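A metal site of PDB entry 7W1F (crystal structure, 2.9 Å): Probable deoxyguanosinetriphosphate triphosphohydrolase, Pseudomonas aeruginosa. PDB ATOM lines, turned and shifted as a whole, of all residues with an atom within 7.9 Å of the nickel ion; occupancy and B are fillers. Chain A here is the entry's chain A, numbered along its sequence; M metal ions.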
ATOM      1  N   GLN A  64      -5.397 -13.725  10.470  1.00  0.00           N
ATOM      2  CA  GLN A  64      -6.055 -13.154  11.628  1.00  0.00           C
ATOM      3  C   GLN A  64      -7.384 -12.522  11.238  1.00  0.00           C
ATOM      4  O   GLN A  64      -8.435 -12.889  11.758  1.00  0.00           O
ATOM      5  CB  GLN A  64      -5.124 -12.151  12.328  1.00  0.00           C
ATOM      6  CG  GLN A  64      -5.778 -11.287  13.377  1.00  0.00           C
ATOM      7  CD  GLN A  64      -5.969 -11.981  14.720  1.00  0.00           C
ATOM      8  OE1 GLN A  64      -5.377 -13.021  14.993  1.00  0.00           O
ATOM      9  NE2 GLN A  64      -6.798 -11.382  15.566  1.00  0.00           N
ATOM     10  N   ARG A  77      -2.058 -14.955  12.874  1.00  0.00           N
ATOM     11  CA  ARG A  77      -2.329 -15.306  14.260  1.00  0.00           C
ATOM     12  C   ARG A  77      -1.037 -15.172  15.066  1.00  0.00           C
ATOM     13  O   ARG A  77      -1.056 -14.733  16.213  1.00  0.00           O
ATOM     14  CB  ARG A  77      -2.922 -16.706  14.349  1.00  0.00           C
ATOM     15  CG  ARG A  77      -4.138 -16.970  13.465  1.00  0.00           C
ATOM     16  CD  ARG A  77      -5.455 -16.561  14.050  1.00  0.00           C
ATOM     17  NE  ARG A  77      -6.321 -17.721  14.060  1.00  0.00           N
ATOM     18  CZ  ARG A  77      -6.930 -18.181  12.985  1.00  0.00           C
ATOM     19  NH1 ARG A  77      -7.696 -19.253  13.112  1.00  0.00           N
ATOM     20  NH2 ARG A  77      -6.715 -17.653  11.789  1.00  0.00           N
ATOM     21  N   HIS A  80      -0.431 -11.375  15.704  1.00  0.00           N
ATOM     22  CA  HIS A  80      -1.380 -10.991  16.753  1.00  0.00           C
ATOM     23  C   HIS A  80      -0.930 -11.532  18.110  1.00  0.00           C
ATOM     24  O   HIS A  80      -0.857 -10.789  19.090  1.00  0.00           O
ATOM     25  CB  HIS A  80      -2.783 -11.490  16.410  1.00  0.00           C
ATOM     26  CG  HIS A  80      -3.691 -11.646  17.606  1.00  0.00           C
ATOM     27  ND1 HIS A  80      -4.022 -10.596  18.434  1.00  0.00           N
ATOM     28  CD2 HIS A  80      -4.355 -12.725  18.079  1.00  0.00           C
ATOM     29  CE1 HIS A  80      -4.836 -11.035  19.382  1.00  0.00           C
ATOM     30  NE2 HIS A  80      -5.050 -12.322  19.190  1.00  0.00           N
ATOM     31  N   SER A  81      -0.607 -12.818  18.158  1.00  0.00           N
ATOM     32  CA  SER A  81      -0.217 -13.437  19.413  1.00  0.00           C
ATOM     33  C   SER A  81       1.059 -12.831  19.979  1.00  0.00           C
ATOM     34  O   SER A  81       1.226 -12.778  21.205  1.00  0.00           O
ATOM     35  CB  SER A  81      -0.063 -14.938  19.223  1.00  0.00           C
ATOM     36  OG  SER A  81      -1.271 -15.507  18.733  1.00  0.00           O
ATOM     37  N   VAL A  84       0.067  -9.660  21.822  1.00  0.00           N
ATOM     38  CA  VAL A  84      -0.581 -10.030  23.074  1.00  0.00           C
ATOM     39  C   VAL A  84       0.465 -10.482  24.093  1.00  0.00           C
ATOM     40  O   VAL A  84       0.339 -10.220  25.288  1.00  0.00           O
ATOM     41  CB  VAL A  84      -1.657 -11.089  22.815  1.00  0.00           C
ATOM     42  CG1 VAL A  84      -2.125 -11.702  24.105  1.00  0.00           C
ATOM     43  CG2 VAL A  84      -2.822 -10.457  22.087  1.00  0.00           C
ATOM     44  N   CYS A 123       0.076 -16.176  26.306  1.00  0.00           N
ATOM     45  CA  CYS A 123      -0.359 -15.295  25.229  1.00  0.00           C
ATOM     46  C   CYS A 123       0.042 -15.845  23.870  1.00  0.00           C
ATOM     47  O   CYS A 123      -0.754 -15.813  22.924  1.00  0.00           O
ATOM     48  CB  CYS A 123       0.264 -13.909  25.406  1.00  0.00           C
ATOM     49  SG  CYS A 123      -0.280 -13.025  26.867  1.00  0.00           S
ATOM     50  N   HIS A 126      -2.244 -18.648  22.975  1.00  0.00           N
ATOM     51  CA  HIS A 126      -3.664 -18.468  23.266  1.00  0.00           C
ATOM     52  C   HIS A 126      -4.542 -18.799  22.081  1.00  0.00           C
ATOM     53  O   HIS A 126      -5.750 -19.006  22.255  1.00  0.00           O
ATOM     54  CB  HIS A 126      -3.927 -17.040  23.755  1.00  0.00           C
ATOM     55  CG  HIS A 126      -4.255 -16.070  22.662  1.00  0.00           C
ATOM     56  ND1 HIS A 126      -3.296 -15.462  21.883  1.00  0.00           N
ATOM     57  CD2 HIS A 126      -5.452 -15.607  22.213  1.00  0.00           C
ATOM     58  CE1 HIS A 126      -3.884 -14.646  21.022  1.00  0.00           C
ATOM     59  NE2 HIS A 126      -5.185 -14.721  21.193  1.00  0.00           N
ATOM     60  N   ASP A 127      -3.970 -18.919  20.889  1.00  0.00           N
ATOM     61  CA  ASP A 127      -4.719 -19.027  19.649  1.00  0.00           C
ATOM     62  C   ASP A 127      -4.305 -20.225  18.811  1.00  0.00           C
ATOM     63  O   ASP A 127      -4.703 -20.318  17.649  1.00  0.00           O
ATOM     64  CB  ASP A 127      -4.517 -17.754  18.820  1.00  0.00           C
ATOM     65  CG  ASP A 127      -5.793 -17.222  18.234  1.00  0.00           C
ATOM     66  OD1 ASP A 127      -6.851 -17.799  18.552  1.00  0.00           O
ATOM     67  OD2 ASP A 127      -5.720 -16.240  17.464  1.00  0.00           O
ATOM     68  N   ASN A 130      -7.758 -22.736  17.821  1.00  0.00           N
ATOM     69  CA  ASN A 130      -8.870 -22.462  16.932  1.00  0.00           C
ATOM     70  C   ASN A 130      -8.468 -22.664  15.464  1.00  0.00           C
ATOM     71  O   ASN A 130      -7.296 -22.467  15.109  1.00  0.00           O
ATOM     72  CB  ASN A 130      -9.468 -21.055  17.172  1.00  0.00           C
ATOM     73  CG  ASN A 130      -8.455 -19.901  17.008  1.00  0.00           C
ATOM     74  OD1 ASN A 130      -8.845 -18.792  16.620  1.00  0.00           O
ATOM     75  ND2 ASN A 130      -7.195 -20.142  17.317  1.00  0.00           N
ATOM     76  N   MET A 259      -3.734 -13.009  30.840  1.00  0.00           N
ATOM     77  CA  MET A 259      -3.722 -13.222  29.393  1.00  0.00           C
ATOM     78  C   MET A 259      -4.976 -12.668  28.728  1.00  0.00           C
ATOM     79  O   MET A 259      -4.904 -12.088  27.642  1.00  0.00           O
ATOM     80  CB  MET A 259      -3.616 -14.705  29.076  1.00  0.00           C
ATOM     81  CG  MET A 259      -3.695 -14.999  27.584  1.00  0.00           C
ATOM     82  SD  MET A 259      -4.891 -16.314  27.241  1.00  0.00           S
ATOM     83  CE  MET A 259      -6.369 -15.376  26.863  1.00  0.00           C
ATOM     84  N   ALA A 262      -4.606  -9.159  28.328  1.00  0.00           N
ATOM     85  CA  ALA A 262      -3.674  -8.932  27.227  1.00  0.00           C
ATOM     86  C   ALA A 262      -4.391  -9.025  25.894  1.00  0.00           C
ATOM     87  O   ALA A 262      -4.251  -8.134  25.042  1.00  0.00           O
ATOM     88  CB  ALA A 262      -2.525  -9.946  27.312  1.00  0.00           C
ATOM     89  N   ASP A 263      -5.160 -10.105  25.685  1.00  0.00           N
ATOM     90  CA  ASP A 263      -5.881 -10.266  24.423  1.00  0.00           C
ATOM     91  C   ASP A 263      -6.903  -9.155  24.225  1.00  0.00           C
ATOM     92  O   ASP A 263      -7.090  -8.676  23.108  1.00  0.00           O
ATOM     93  CB  ASP A 263      -6.568 -11.627  24.364  1.00  0.00           C
ATOM     94  CG  ASP A 263      -7.129 -11.955  22.979  1.00  0.00           C
ATOM     95  OD1 ASP A 263      -6.347 -12.311  22.065  1.00  0.00           O
ATOM     96  OD2 ASP A 263      -8.352 -11.828  22.801  1.00  0.00           O
ATOM     97  N   ASP A 264      -7.561  -8.733  25.306  1.00  0.00           N
ATOM     98  CA  ASP A 264      -8.549  -7.648  25.198  1.00  0.00           C
ATOM     99  C   ASP A 264      -7.907  -6.343  24.740  1.00  0.00           C
ATOM    100  O   ASP A 264      -8.485  -5.610  23.938  1.00  0.00           O
ATOM    101  CB  ASP A 264      -9.254  -7.459  26.536  1.00  0.00           C
ATOM    102  CG  ASP A 264     -10.373  -8.453  26.750  1.00  0.00           C
ATOM    103  OD1 ASP A 264     -11.163  -8.656  25.798  1.00  0.00           O
ATOM    104  OD2 ASP A 264     -10.457  -9.040  27.853  1.00  0.00           O
ATOM    105  N   SER A 266      -5.015  -5.673  23.023  1.00  0.00           N
ATOM    106  CA  SER A 266      -4.527  -5.682  21.654  1.00  0.00           C
ATOM    107  C   SER A 266      -5.449  -6.448  20.724  1.00  0.00           C
ATOM    108  O   SER A 266      -5.033  -6.839  19.631  1.00  0.00           O
ATOM    109  CB  SER A 266      -3.107  -6.253  21.602  1.00  0.00           C
ATOM    110  OG  SER A 266      -2.785  -6.931  22.809  1.00  0.00           O
ATOM    111  N   TYR A 267      -6.701  -6.662  21.146  1.00  0.00           N
ATOM    112  CA  TYR A 267      -7.689  -7.382  20.352  1.00  0.00           C
ATOM    113  C   TYR A 267      -7.872  -6.759  18.972  1.00  0.00           C
ATOM    114  O   TYR A 267      -7.779  -7.451  17.961  1.00  0.00           O
ATOM    115  CB  TYR A 267      -9.015  -7.391  21.130  1.00  0.00           C
ATOM    116  CG  TYR A 267     -10.187  -8.245  20.644  1.00  0.00           C
ATOM    117  CD1 TYR A 267     -10.561  -8.296  19.301  1.00  0.00           C
ATOM    118  CD2 TYR A 267     -10.983  -8.946  21.555  1.00  0.00           C
ATOM    119  CE1 TYR A 267     -11.648  -9.037  18.877  1.00  0.00           C
ATOM    120  CE2 TYR A 267     -12.075  -9.690  21.145  1.00  0.00           C
ATOM    121  CZ  TYR A 267     -12.405  -9.729  19.804  1.00  0.00           C
ATOM    122  OH  TYR A 267     -13.488 -10.468  19.390  1.00  0.00           O
ATOM    123  N   ASP A 271      -5.723  -4.739  14.291  1.00  0.00           N
ATOM    124  CA  ASP A 271      -6.481  -4.987  13.063  1.00  0.00           C
ATOM    125  C   ASP A 271      -6.919  -3.683  12.410  1.00  0.00           C
ATOM    126  O   ASP A 271      -6.968  -3.596  11.172  1.00  0.00           O
ATOM    127  CB  ASP A 271      -7.665  -5.912  13.364  1.00  0.00           C
ATOM    128  CG  ASP A 271      -7.221  -7.283  13.887  1.00  0.00           C
ATOM    129  OD1 ASP A 271      -6.072  -7.695  13.577  1.00  0.00           O
ATOM    130  OD2 ASP A 271      -8.001  -7.956  14.589  1.00  0.00           O
HETATM  131 NI    NI M   1      -6.585 -13.211  20.275  1.00  0.00          NI
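The backbone carbonyl oxygen (O) of Cys 123 sits at hydrogen-bond distance from a ring nitrogen (ND1) of His 126 (2.8 Å).
Within 4 Å of the nickel ion: His 80, His 126 and Asp 263. The nearest printed residue that does not touch the nickel ion is Asp 127 (4.2 Å).
The side-chain carboxylate (OD1) of Asp 263 binds the nickel ion, at 2.0 Å. NE2 of His 80 is bound to the nickel ion (2.1 Å). A ring nitrogen (NE2) of His 126 binds the nickel ion.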
